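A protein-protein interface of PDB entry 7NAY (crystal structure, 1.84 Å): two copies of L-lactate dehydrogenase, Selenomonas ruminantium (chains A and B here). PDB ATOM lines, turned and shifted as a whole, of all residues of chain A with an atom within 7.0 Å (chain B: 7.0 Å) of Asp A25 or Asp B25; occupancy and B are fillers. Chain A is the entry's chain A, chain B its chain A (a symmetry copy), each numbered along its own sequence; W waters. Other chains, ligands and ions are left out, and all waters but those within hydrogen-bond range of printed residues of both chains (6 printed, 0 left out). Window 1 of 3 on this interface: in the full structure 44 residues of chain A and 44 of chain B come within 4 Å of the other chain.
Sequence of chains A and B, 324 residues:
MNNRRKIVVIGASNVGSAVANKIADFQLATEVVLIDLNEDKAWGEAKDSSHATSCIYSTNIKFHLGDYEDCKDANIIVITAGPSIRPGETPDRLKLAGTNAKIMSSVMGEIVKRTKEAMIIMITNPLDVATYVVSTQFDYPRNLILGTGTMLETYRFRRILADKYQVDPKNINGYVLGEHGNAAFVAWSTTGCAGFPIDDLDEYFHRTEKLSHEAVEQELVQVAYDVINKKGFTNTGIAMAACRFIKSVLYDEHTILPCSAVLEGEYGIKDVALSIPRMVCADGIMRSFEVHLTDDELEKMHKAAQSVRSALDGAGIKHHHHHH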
ATOM      1  N   ALA A  18      -0.263   5.806  16.855  1.00  0.00           N
ATOM      2  CA  ALA A  18       0.583   5.115  17.863  1.00  0.00           C
ATOM      3  C   ALA A  18       0.367   5.724  19.256  1.00  0.00           C
ATOM      4  O   ALA A  18       0.200   4.977  20.264  1.00  0.00           O
ATOM      5  CB  ALA A  18       2.018   5.152  17.425  1.00  0.00           C
ATOM      6  N   VAL A  19       0.281   7.036  19.356  1.00  0.00           N
ATOM      7  CA  VAL A  19       0.036   7.691  20.669  1.00  0.00           C
ATOM      8  C   VAL A  19      -1.350   7.228  21.169  1.00  0.00           C
ATOM      9  O   VAL A  19      -1.497   6.795  22.344  1.00  0.00           O
ATOM     10  CB  VAL A  19       0.100   9.217  20.508  1.00  0.00           C
ATOM     11  CG1 VAL A  19      -0.545   9.889  21.698  1.00  0.00           C
ATOM     12  CG2 VAL A  19       1.526   9.700  20.237  1.00  0.00           C
ATOM     13  N   ALA A  20      -2.353   7.295  20.300  1.00  0.00           N
ATOM     14  CA  ALA A  20      -3.748   6.954  20.649  1.00  0.00           C
ATOM     15  C   ALA A  20      -3.813   5.506  21.125  1.00  0.00           C
ATOM     16  O   ALA A  20      -4.572   5.231  22.094  1.00  0.00           O
ATOM     17  CB  ALA A  20      -4.683   7.173  19.474  1.00  0.00           C
ATOM     18  N   ASN A  21      -3.113   4.608  20.426  1.00  0.00           N
ATOM     19  CA  ASN A  21      -3.161   3.151  20.730  1.00  0.00           C
ATOM     20  C   ASN A  21      -2.379   2.808  22.011  1.00  0.00           C
ATOM     21  O   ASN A  21      -2.795   1.887  22.712  1.00  0.00           O
ATOM     22  CB  ASN A  21      -2.910   2.343  19.464  1.00  0.00           C
ATOM     23  CG  ASN A  21      -4.080   2.433  18.513  1.00  0.00           C
ATOM     24  OD1 ASN A  21      -3.907   2.621  17.316  1.00  0.00           O
ATOM     25  ND2 ASN A  21      -5.279   2.314  19.051  1.00  0.00           N
ATOM     26  N   LYS A  22      -1.265   3.495  22.266  1.00  0.00           N
ATOM     27  CA  LYS A  22      -0.579   3.332  23.564  1.00  0.00           C
ATOM     28  C   LYS A  22      -1.513   3.811  24.692  1.00  0.00           C
ATOM     29  O   LYS A  22      -1.619   3.120  25.738  1.00  0.00           O
ATOM     30  CB  LYS A  22       0.823   3.957  23.578  1.00  0.00           C
ATOM     31  CG  LYS A  22       1.840   3.173  22.749  1.00  0.00           C
ATOM     32  CD  LYS A  22       3.237   3.133  23.312  1.00  0.00           C
ATOM     33  CE  LYS A  22       4.271   2.439  22.462  1.00  0.00           C
ATOM     34  NZ  LYS A  22       4.021   0.988  22.253  1.00  0.00           N
ATOM     35  N   ILE A  23      -2.135   4.978  24.535  1.00  0.00           N
ATOM     36  CA  ILE A  23      -3.131   5.478  25.510  1.00  0.00           C
ATOM     37  C   ILE A  23      -4.175   4.371  25.757  1.00  0.00           C
ATOM     38  O   ILE A  23      -4.523   4.138  26.908  1.00  0.00           O
ATOM     39  CB  ILE A  23      -3.787   6.781  25.010  1.00  0.00           C
ATOM     40  CG1 ILE A  23      -2.793   7.940  25.107  1.00  0.00           C
ATOM     41  CG2 ILE A  23      -5.072   7.020  25.761  1.00  0.00           C
ATOM     42  CD1 ILE A  23      -3.219   9.228  24.406  1.00  0.00           C
ATOM     43  N   ALA A  24      -4.677   3.729  24.697  1.00  0.00           N
ATOM     44  CA  ALA A  24      -5.731   2.722  24.852  1.00  0.00           C
ATOM     45  C   ALA A  24      -5.149   1.494  25.583  1.00  0.00           C
ATOM     46  O   ALA A  24      -5.792   0.991  26.546  1.00  0.00           O
ATOM     47  CB  ALA A  24      -6.318   2.409  23.505  1.00  0.00           C
ATOM     48  N   ASP A  25      -3.943   1.083  25.208  1.00  0.00           N
ATOM     49  CA  ASP A  25      -3.309  -0.125  25.809  1.00  0.00           C
ATOM     50  C   ASP A  25      -3.134   0.093  27.322  1.00  0.00           C
ATOM     51  O   ASP A  25      -3.501  -0.802  28.136  1.00  0.00           O
ATOM     52  CB  ASP A  25      -2.006  -0.453  25.083  1.00  0.00           C
ATOM     53  CG  ASP A  25      -2.157  -1.130  23.739  1.00  0.00           C
ATOM     54  OD1 ASP A  25      -3.287  -1.496  23.365  1.00  0.00           O
ATOM     55  OD2 ASP A  25      -1.139  -1.294  23.087  1.00  0.00           O
ATOM     56  N   PHE A  26      -2.656   1.270  27.712  1.00  0.00           N
ATOM     57  CA  PHE A  26      -2.374   1.578  29.133  1.00  0.00           C
ATOM     58  C   PHE A  26      -3.625   2.097  29.837  1.00  0.00           C
ATOM     59  O   PHE A  26      -3.482   2.449  31.027  1.00  0.00           O
ATOM     60  CB  PHE A  26      -1.206   2.560  29.206  1.00  0.00           C
ATOM     61  CG  PHE A  26       0.056   1.972  28.617  1.00  0.00           C
ATOM     62  CD1 PHE A  26       0.488   0.721  29.017  1.00  0.00           C
ATOM     63  CD2 PHE A  26       0.808   2.658  27.682  1.00  0.00           C
ATOM     64  CE1 PHE A  26       1.646   0.167  28.479  1.00  0.00           C
ATOM     65  CE2 PHE A  26       1.948   2.085  27.134  1.00  0.00           C
ATOM     66  CZ  PHE A  26       2.365   0.859  27.556  1.00  0.00           C
ATOM     67  N   GLN A  27      -4.752   2.195  29.119  1.00  0.00           N
ATOM     68  CA  GLN A  27      -6.069   2.585  29.673  1.00  0.00           C
ATOM     69  C   GLN A  27      -5.948   3.971  30.343  1.00  0.00           C
ATOM     70  O   GLN A  27      -6.465   4.186  31.464  1.00  0.00           O
ATOM     71  CB  GLN A  27      -6.575   1.472  30.596  1.00  0.00           C
ATOM     72  CG  GLN A  27      -6.580   0.097  29.941  1.00  0.00           C
ATOM     73  CD  GLN A  27      -7.346  -0.955  30.718  1.00  0.00           C
ATOM     74  OE1 GLN A  27      -7.936  -0.703  31.773  1.00  0.00           O
ATOM     75  NE2 GLN A  27      -7.380  -2.166  30.177  1.00  0.00           N
ATOM     76  N   LEU A  28      -5.365   4.944  29.633  1.00  0.00           N
ATOM     77  CA  LEU A  28      -5.074   6.279  30.184  1.00  0.00           C
ATOM     78  C   LEU A  28      -6.213   7.260  29.911  1.00  0.00           C
ATOM     79  O   LEU A  28      -6.055   8.442  30.299  1.00  0.00           O
ATOM     80  CB  LEU A  28      -3.778   6.772  29.547  1.00  0.00           C
ATOM     81  CG  LEU A  28      -2.546   5.958  29.942  1.00  0.00           C
ATOM     82  CD1 LEU A  28      -1.283   6.579  29.336  1.00  0.00           C
ATOM     83  CD2 LEU A  28      -2.456   5.828  31.450  1.00  0.00           C
ATOM     84  N   ALA A  52     -10.363  -3.022  18.958  1.00  0.00           N
ATOM     85  CA  ALA A  52      -9.386  -3.409  19.999  1.00  0.00           C
ATOM     86  C   ALA A  52     -10.013  -3.168  21.361  1.00  0.00           C
ATOM     87  O   ALA A  52      -9.834  -4.053  22.218  1.00  0.00           O
ATOM     88  CB  ALA A  52      -8.043  -2.695  19.872  1.00  0.00           C
ATOM     89  N   THR A  53     -10.782  -2.085  21.574  1.00  0.00           N
ATOM     90  CA  THR A  53     -11.273  -1.759  22.933  1.00  0.00           C
ATOM     91  C   THR A  53     -12.573  -2.520  23.237  1.00  0.00           C
ATOM     92  O   THR A  53     -13.188  -2.266  24.276  1.00  0.00           O
ATOM     93  CB  THR A  53     -11.388  -0.251  23.144  1.00  0.00           C
ATOM     94  OG1 THR A  53     -12.446   0.222  22.298  1.00  0.00           O
ATOM     95  CG2 THR A  53     -10.038   0.400  22.907  1.00  0.00           C
ATOM     96  N   TYR A  57     -10.207  -7.891  27.897  1.00  0.00           N
ATOM     97  CA  TYR A  57      -9.177  -7.302  28.788  1.00  0.00           C
ATOM     98  C   TYR A  57      -9.084  -5.778  28.602  1.00  0.00           C
ATOM     99  O   TYR A  57      -8.364  -5.112  29.377  1.00  0.00           O
ATOM    100  CB  TYR A  57      -7.821  -7.995  28.608  1.00  0.00           C
ATOM    101  CG  TYR A  57      -7.765  -9.410  29.122  1.00  0.00           C
ATOM    102  CD1 TYR A  57      -8.328  -9.764  30.337  1.00  0.00           C
ATOM    103  CD2 TYR A  57      -7.181 -10.416  28.384  1.00  0.00           C
ATOM    104  CE1 TYR A  57      -8.321 -11.069  30.793  1.00  0.00           C
ATOM    105  CE2 TYR A  57      -7.158 -11.732  28.824  1.00  0.00           C
ATOM    106  CZ  TYR A  57      -7.707 -12.062  30.040  1.00  0.00           C
ATOM    107  OH  TYR A  57      -7.655 -13.369  30.447  1.00  0.00           O
ATOM    108  N   SER A  58      -9.860  -5.189  27.711  1.00  0.00           N
ATOM    109  CA  SER A  58      -9.857  -3.712  27.559  1.00  0.00           C
ATOM    110  C   SER A  58     -11.003  -3.106  28.358  1.00  0.00           C
ATOM    111  O   SER A  58     -12.093  -3.684  28.355  1.00  0.00           O
ATOM    112  CB  SER A  58      -9.982  -3.311  26.123  1.00  0.00           C
ATOM    113  OG  SER A  58      -9.752  -1.941  25.995  1.00  0.00           O
ATOM    114  N   ILE A  61     -13.125   1.850  26.091  1.00  0.00           N
ATOM    115  CA  ILE A  61     -12.591   3.188  25.702  1.00  0.00           C
ATOM    116  C   ILE A  61     -13.252   3.609  24.401  1.00  0.00           C
ATOM    117  O   ILE A  61     -13.253   2.844  23.444  1.00  0.00           O
ATOM    118  CB  ILE A  61     -11.071   3.195  25.617  1.00  0.00           C
ATOM    119  CG1 ILE A  61     -10.462   2.833  26.973  1.00  0.00           C
ATOM    120  CG2 ILE A  61     -10.578   4.539  25.096  1.00  0.00           C
ATOM    121  CD1 ILE A  61      -8.956   2.652  26.945  1.00  0.00           C
ATOM    122  N   PHE A  63     -13.483   5.451  21.147  1.00  0.00           N
ATOM    123  CA  PHE A  63     -12.669   6.059  20.069  1.00  0.00           C
ATOM    124  C   PHE A  63     -13.600   6.659  19.026  1.00  0.00           C
ATOM    125  O   PHE A  63     -14.519   5.933  18.581  1.00  0.00           O
ATOM    126  CB  PHE A  63     -11.822   5.004  19.370  1.00  0.00           C
ATOM    127  CG  PHE A  63     -10.465   4.846  19.994  1.00  0.00           C
ATOM    128  CD1 PHE A  63     -10.299   4.110  21.147  1.00  0.00           C
ATOM    129  CD2 PHE A  63      -9.372   5.501  19.458  1.00  0.00           C
ATOM    130  CE1 PHE A  63      -9.033   3.944  21.687  1.00  0.00           C
ATOM    131  CE2 PHE A  63      -8.123   5.383  20.042  1.00  0.00           C
ATOM    132  CZ  PHE A  63      -7.954   4.598  21.147  1.00  0.00           C
ATOM    133  N   THR A 236       6.869   4.520  17.591  1.00  0.00           N
ATOM    134  CA  THR A 236       6.723   3.703  18.824  1.00  0.00           C
ATOM    135  C   THR A 236       7.344   4.414  20.032  1.00  0.00           C
ATOM    136  O   THR A 236       6.666   4.571  21.038  1.00  0.00           O
ATOM    137  CB  THR A 236       7.211   2.267  18.581  1.00  0.00           C
ATOM    138  OG1 THR A 236       6.727   1.789  17.329  1.00  0.00           O
ATOM    139  CG2 THR A 236       6.850   1.326  19.710  1.00  0.00           C
ATOM    140  N   MET A 240       5.417   6.167  23.358  1.00  0.00           N
ATOM    141  CA  MET A 240       5.784   5.779  24.720  1.00  0.00           C
ATOM    142  C   MET A 240       6.103   7.046  25.507  1.00  0.00           C
ATOM    143  O   MET A 240       5.552   7.187  26.632  1.00  0.00           O
ATOM    144  CB  MET A 240       6.951   4.789  24.771  1.00  0.00           C
ATOM    145  CG  MET A 240       7.089   4.129  26.137  1.00  0.00           C
ATOM    146  SD  MET A 240       5.678   3.003  26.346  1.00  0.00           S
ATOM    147  CE  MET A 240       6.410   1.578  27.157  1.00  0.00           C
ATOM    148  N   ALA B  18       2.289  -3.719  14.817  1.00  0.00           N
ATOM    149  CA  ALA B  18       1.179  -3.521  15.786  1.00  0.00           C
ATOM    150  C   ALA B  18       1.082  -4.718  16.744  1.00  0.00           C
ATOM    151  O   ALA B  18       0.948  -4.533  17.989  1.00  0.00           O
ATOM    152  CB  ALA B  18      -0.098  -3.263  15.042  1.00  0.00           C
ATOM    153  N   VAL B  19       1.221  -5.929  16.244  1.00  0.00           N
ATOM    154  CA  VAL B  19       1.175  -7.131  17.120  1.00  0.00           C
ATOM    155  C   VAL B  19       2.362  -7.038  18.102  1.00  0.00           C
ATOM    156  O   VAL B  19       2.188  -7.207  19.339  1.00  0.00           O
ATOM    157  CB  VAL B  19       1.247  -8.402  16.261  1.00  0.00           C
ATOM    158  CG1 VAL B  19       1.617  -9.587  17.124  1.00  0.00           C
ATOM    159  CG2 VAL B  19      -0.037  -8.617  15.455  1.00  0.00           C
ATOM    160  N   ALA B  20       3.552  -6.757  17.579  1.00  0.00           N
ATOM    161  CA  ALA B  20       4.793  -6.703  18.377  1.00  0.00           C
ATOM    162  C   ALA B  20       4.649  -5.646  19.469  1.00  0.00           C
ATOM    163  O   ALA B  20       5.127  -5.898  20.609  1.00  0.00           O
ATOM    164  CB  ALA B  20       6.001  -6.411  17.507  1.00  0.00           C
ATOM    165  N   ASN B  21       4.089  -4.486  19.116  1.00  0.00           N
ATOM    166  CA  ASN B  21       3.971  -3.340  20.060  1.00  0.00           C
ATOM    167  C   ASN B  21       2.877  -3.581  21.117  1.00  0.00           C
ATOM    168  O   ASN B  21       3.050  -3.116  22.243  1.00  0.00           O
ATOM    169  CB  ASN B  21       3.991  -2.025  19.294  1.00  0.00           C
ATOM    170  CG  ASN B  21       5.363  -1.737  18.731  1.00  0.00           C
ATOM    171  OD1 ASN B  21       5.503  -1.339  17.582  1.00  0.00           O
ATOM    172  ND2 ASN B  21       6.382  -1.954  19.540  1.00  0.00           N
ATOM    173  N   LYS B  22       1.780  -4.237  20.741  1.00  0.00           N
ATOM    174  CA  LYS B  22       0.785  -4.651  21.753  1.00  0.00           C
ATOM    175  C   LYS B  22       1.440  -5.655  22.722  1.00  0.00           C
ATOM    176  O   LYS B  22       1.241  -5.533  23.959  1.00  0.00           O
ATOM    177  CB  LYS B  22      -0.535  -5.125  21.129  1.00  0.00           C
ATOM    178  CG  LYS B  22      -1.363  -3.985  20.535  1.00  0.00           C
ATOM    179  CD  LYS B  22      -2.855  -4.124  20.688  1.00  0.00           C
ATOM    180  CE  LYS B  22      -3.688  -3.053  20.030  1.00  0.00           C
ATOM    181  NZ  LYS B  22      -3.484  -1.688  20.583  1.00  0.00           N
ATOM    182  N   ILE B  23       2.152  -6.652  22.202  1.00  0.00           N
ATOM    183  CA  ILE B  23       2.905  -7.606  23.048  1.00  0.00           C
ATOM    184  C   ILE B  23       3.786  -6.807  24.028  1.00  0.00           C
ATOM    185  O   ILE B  23       3.824  -7.154  25.202  1.00  0.00           O
ATOM    186  CB  ILE B  23       3.743  -8.568  22.181  1.00  0.00           C
ATOM    187  CG1 ILE B  23       2.830  -9.578  21.483  1.00  0.00           C
ATOM    188  CG2 ILE B  23       4.815  -9.206  23.028  1.00  0.00           C
ATOM    189  CD1 ILE B  23       3.495 -10.418  20.395  1.00  0.00           C
ATOM    190  N   ALA B  24       4.493  -5.779  23.546  1.00  0.00           N
ATOM    191  CA  ALA B  24       5.412  -5.025  24.404  1.00  0.00           C
ATOM    192  C   ALA B  24       4.593  -4.241  25.451  1.00  0.00           C
ATOM    193  O   ALA B  24       4.946  -4.281  26.662  1.00  0.00           O
ATOM    194  CB  ALA B  24       6.294  -4.162  23.546  1.00  0.00           C
ATOM    195  N   ASP B  25       3.494  -3.629  25.023  1.00  0.00           N
ATOM    196  CA  ASP B  25       2.658  -2.800  25.937  1.00  0.00           C
ATOM    197  C   ASP B  25       2.129  -3.682  27.081  1.00  0.00           C
ATOM    198  O   ASP B  25       2.228  -3.288  28.279  1.00  0.00           O
ATOM    199  CB  ASP B  25       1.557  -2.094  25.149  1.00  0.00           C
ATOM    200  CG  ASP B  25       1.993  -0.882  24.354  1.00  0.00           C
ATOM    201  OD1 ASP B  25       3.156  -0.455  24.484  1.00  0.00           O
ATOM    202  OD2 ASP B  25       1.159  -0.373  23.623  1.00  0.00           O
ATOM    203  N   PHE B  26       1.643  -4.873  26.751  1.00  0.00           N
ATOM    204  CA  PHE B  26       1.038  -5.785  27.749  1.00  0.00           C
ATOM    205  C   PHE B  26       2.106  -6.647  28.418  1.00  0.00           C
ATOM    206  O   PHE B  26       1.696  -7.499  29.233  1.00  0.00           O
ATOM    207  CB  PHE B  26      -0.048  -6.616  27.070  1.00  0.00           C
ATOM    208  CG  PHE B  26      -1.160  -5.745  26.528  1.00  0.00           C
ATOM    209  CD1 PHE B  26      -1.753  -4.797  27.340  1.00  0.00           C
ATOM    210  CD2 PHE B  26      -1.614  -5.873  25.229  1.00  0.00           C
ATOM    211  CE1 PHE B  26      -2.775  -3.987  26.852  1.00  0.00           C
ATOM    212  CE2 PHE B  26      -2.617  -5.043  24.745  1.00  0.00           C
ATOM    213  CZ  PHE B  26      -3.200  -4.128  25.568  1.00  0.00           C
ATOM    214  N   GLN B  27       3.380  -6.471  28.040  1.00  0.00           N
ATOM    215  CA  GLN B  27       4.540  -7.154  28.656  1.00  0.00           C
ATOM    216  C   GLN B  27       4.344  -8.682  28.556  1.00  0.00           C
ATOM    217  O   GLN B  27       4.580  -9.422  29.539  1.00  0.00           O
ATOM    218  CB  GLN B  27       4.733  -6.627  30.081  1.00  0.00           C
ATOM    219  CG  GLN B  27       4.815  -5.108  30.161  1.00  0.00           C
ATOM    220  CD  GLN B  27       5.299  -4.584  31.498  1.00  0.00           C
ATOM    221  OE1 GLN B  27       5.625  -5.331  32.426  1.00  0.00           O
ATOM    222  NE2 GLN B  27       5.391  -3.265  31.605  1.00  0.00           N
ATOM    223  N   LEU B  28       4.015  -9.179  27.357  1.00  0.00           N
ATOM    224  CA  LEU B  28       3.679 -10.596  27.137  1.00  0.00           C
ATOM    225  C   LEU B  28       4.909 -11.407  26.733  1.00  0.00           C
ATOM    226  O   LEU B  28       4.734 -12.623  26.478  1.00  0.00           O
ATOM    227  CB  LEU B  28       2.614 -10.658  26.047  1.00  0.00           C
ATOM    228  CG  LEU B  28       1.275 -10.044  26.456  1.00  0.00           C
ATOM    229  CD1 LEU B  28       0.242 -10.235  25.341  1.00  0.00           C
ATOM    230  CD2 LEU B  28       0.808 -10.621  27.778  1.00  0.00           C
ATOM    231  N   ALA B  52      10.993   2.496  23.184  1.00  0.00           N
ATOM    232  CA  ALA B  52       9.767   2.417  24.007  1.00  0.00           C
ATOM    233  C   ALA B  52      10.052   1.536  25.211  1.00  0.00           C
ATOM    234  O   ALA B  52       9.613   1.932  26.306  1.00  0.00           O
ATOM    235  CB  ALA B  52       8.544   1.926  23.238  1.00  0.00           C
ATOM    236  N   THR B  53      10.810   0.431  25.082  1.00  0.00           N
ATOM    237  CA  THR B  53      10.969  -0.515  26.209  1.00  0.00           C
ATOM    238  C   THR B  53      12.105  -0.064  27.141  1.00  0.00           C
ATOM    239  O   THR B  53      12.458  -0.806  28.061  1.00  0.00           O
ATOM    240  CB  THR B  53      11.122  -1.954  25.721  1.00  0.00           C
ATOM    241  OG1 THR B  53      12.382  -2.047  25.043  1.00  0.00           O
ATOM    242  CG2 THR B  53       9.914  -2.337  24.884  1.00  0.00           C
ATOM    243  N   TYR B  57       8.335   2.679  33.009  1.00  0.00           N
ATOM    244  CA  TYR B  57       7.155   1.810  33.241  1.00  0.00           C
ATOM    245  C   TYR B  57       7.205   0.553  32.355  1.00  0.00           C
ATOM    246  O   TYR B  57       6.358  -0.350  32.530  1.00  0.00           O
ATOM    247  CB  TYR B  57       5.845   2.589  33.073  1.00  0.00           C
ATOM    248  CG  TYR B  57       5.577   3.607  34.151  1.00  0.00           C
ATOM    249  CD1 TYR B  57       5.799   3.323  35.488  1.00  0.00           C
ATOM    250  CD2 TYR B  57       5.133   4.874  33.844  1.00  0.00           C
ATOM    251  CE1 TYR B  57       5.600   4.267  36.479  1.00  0.00           C
ATOM    252  CE2 TYR B  57       4.921   5.836  34.821  1.00  0.00           C
ATOM    253  CZ  TYR B  57       5.131   5.532  36.145  1.00  0.00           C
ATOM    254  OH  TYR B  57       4.900   6.503  37.083  1.00  0.00           O
ATOM    255  N   SER B  58       8.211   0.397  31.515  1.00  0.00           N
ATOM    256  CA  SER B  58       8.338  -0.840  30.703  1.00  0.00           C
ATOM    257  C   SER B  58       9.286  -1.816  31.386  1.00  0.00           C
ATOM    258  O   SER B  58      10.304  -1.370  31.920  1.00  0.00           O
ATOM    259  CB  SER B  58       8.837  -0.538  29.325  1.00  0.00           C
ATOM    260  OG  SER B  58       8.731  -1.677  28.526  1.00  0.00           O
ATOM    261  N   ILE B  61      12.203  -5.282  27.687  1.00  0.00           N
ATOM    262  CA  ILE B  61      11.865  -6.253  26.606  1.00  0.00           C
ATOM    263  C   ILE B  61      12.852  -6.065  25.467  1.00  0.00           C
ATOM    264  O   ILE B  61      13.042  -4.946  25.005  1.00  0.00           O
ATOM    265  CB  ILE B  61      10.417  -6.127  26.154  1.00  0.00           C
ATOM    266  CG1 ILE B  61       9.471  -6.395  27.327  1.00  0.00           C
ATOM    267  CG2 ILE B  61      10.151  -7.044  24.968  1.00  0.00           C
ATOM    268  CD1 ILE B  61       8.010  -6.129  27.015  1.00  0.00           C
ATOM    269  N   PHE B  63      13.992  -6.204  21.901  1.00  0.00           N
ATOM    270  CA  PHE B  63      13.508  -6.193  20.500  1.00  0.00           C
ATOM    271  C   PHE B  63      14.704  -6.299  19.565  1.00  0.00           C
ATOM    272  O   PHE B  63      15.657  -5.508  19.748  1.00  0.00           O
ATOM    273  CB  PHE B  63      12.797  -4.884  20.184  1.00  0.00           C
ATOM    274  CG  PHE B  63      11.321  -4.950  20.454  1.00  0.00           C
ATOM    275  CD1 PHE B  63      10.830  -4.821  21.735  1.00  0.00           C
ATOM    276  CD2 PHE B  63      10.436  -5.214  19.424  1.00  0.00           C
ATOM    277  CE1 PHE B  63       9.462  -4.846  21.959  1.00  0.00           C
ATOM    278  CE2 PHE B  63       9.077  -5.302  19.667  1.00  0.00           C
ATOM    279  CZ  PHE B  63       8.593  -5.108  20.929  1.00  0.00           C
ATOM    280  N   THR B 236      -4.869  -2.482  14.278  1.00  0.00           N
ATOM    281  CA  THR B 236      -5.082  -2.338  15.741  1.00  0.00           C
ATOM    282  C   THR B 236      -5.938  -3.487  16.288  1.00  0.00           C
ATOM    283  O   THR B 236      -5.521  -4.133  17.239  1.00  0.00           O
ATOM    284  CB  THR B 236      -5.584  -0.926  16.078  1.00  0.00           C
ATOM    285  OG1 THR B 236      -4.835   0.047  15.352  1.00  0.00           O
ATOM    286  CG2 THR B 236      -5.571  -0.637  17.563  1.00  0.00           C
ATOM    287  N   MET B 240      -4.787  -6.694  18.786  1.00  0.00           N
ATOM    288  CA  MET B 240      -5.502  -6.958  20.035  1.00  0.00           C
ATOM    289  C   MET B 240      -5.927  -8.423  20.041  1.00  0.00           C
ATOM    290  O   MET B 240      -5.664  -9.102  21.069  1.00  0.00           O
ATOM    291  CB  MET B 240      -6.705  -6.034  20.247  1.00  0.00           C
ATOM    292  CG  MET B 240      -7.216  -6.073  21.682  1.00  0.00           C
ATOM    293  SD  MET B 240      -5.973  -5.261  22.729  1.00  0.00           S
ATOM    294  CE  MET B 240      -6.969  -4.330  23.898  1.00  0.00           C
HETATM  295  O   HOH W   1      -5.758  -0.102  20.595  1.00  0.00           O
HETATM  296  O   HOH W   2      -6.003   2.576  15.251  1.00  0.00           O
HETATM  297  O   HOH W   3       8.037  -0.474  16.362  1.00  0.00           O
HETATM  298  O   HOH W   4       6.316  -0.560  22.091  1.00  0.00           O
HETATM  299  O   HOH W   5       4.042   1.741  17.387  1.00  0.00           O
HETATM  300  O   HOH W   6      -2.256  -0.103  16.087  1.00  0.00           O
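Printed residues of chain A that touch a printed residue of chain B: Asn A21, Lys A22, Asp A25, Phe A26, Ala A52, Ser A58, Thr A236 and Met A240. Hydrophobic or aromatic side chains of chain B that line the printed part of chain A: Phe B26, Ala B52 and Met B240. Among the printed residues, 13 pairs touch across the chains. Among the printed residues, Asp or Glu carboxylates within 4 Å of a Lys or Arg side-chain nitrogen of the other chain: Lys A22 with Asp B25 and Asp A25 with Lys B22.
Water W6 lies within hydrogen-bond range of OG1 of Thr B236 (2.7 Å) and OD1 of Asn A21 (3.4 Å). Water W5 bridges OG1 of Thr A236 (2.7 Å) and OD1 of Asn B21 (3.4 Å). Water W4 lies within hydrogen-bond range of the side-chain amino group of Lys A22 (2.8 Å) and the side-chain amide nitrogen of Asn B21 (2.9 Å). Water W1 bridges NZ of Lys B22 and ND2 of Asn A21. Water W2 bridges the side-chain hydroxyl (OG1) of Thr B236 (2.8 Å) and the side-chain amide oxygen (OD1) of Asn A21 (2.9 Å). Water W3 bridges the side-chain hydroxyl of Thr A236 (2.8 Å) and the side-chain amide oxygen of Asn B21 (2.9 Å).
OD1 of Asn A21 lies within hydrogen-bond range of OG1 of Thr B236, at 3.4 Å. The side-chain carboxylate (OD1) of Asp B25 lies within salt-bridge range of the side-chain amino group (NZ) of Lys A22, 2.8 Å away. OD1 of Asp A25 is in salt-bridge range of NZ of Lys B22 (2.8 Å). The side-chain carboxylate (OD2) of Asp A25 sits close to the side-chain carboxylate (OD2) of Asp B25 (2.5 Å). The side-chain hydroxyl (OG1) of Thr A236 is in hydrogen-bond range of the side-chain amide oxygen (OD1) of Asn B21, at 3.4 Å.
Ala A20 touches none of the printed residues of chain B. Printed residues of chain B within 4 Å of Phe A26: Asp B25 (3.4 Å). Thr A53 touches none of the printed residues of chain B. Of the printed residues of chain A, Phe B26 touches Asp A25. The nearest printed residue of chain B that does not touch Asp A25 is Asn B21 (4.6 Å).
Asn A21 touches Thr B236, and with the chains exchanged Thr A236 touches Asn B21. Lys A22 touches Asp B25, and with the chains exchanged Asp A25 touches Lys B22. Asp A25 touches Phe B26, and with the chains exchanged Phe A26 touches Asp B25. Ala A52 touches Met B240, and with the chains exchanged Met A240 touches Ala B52. Of the 13 pairs that touch across the chains among the printed residues, 13 have their exchanged pair printed and touching as well.
CZ of Phe B26 touches OD1 of Asp A25, at 3.4 Å. OD1 of Asp B25 touches CZ of Phe A26, 3.4 Å away. O of Thr B236 touches CB of Ala A52, 3.9 Å away. Ala A52 touches Met B240 (O to CE, 3.3 Å). Ser A58 touches Met B240 (CB to CE, 3.9 Å). Ala B52 touches Thr A236. Ala B52 touches Met A240 (O to CE, 3.3 Å). CE of Met A240 touches CB of Ser B58, 3.9 Å away.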
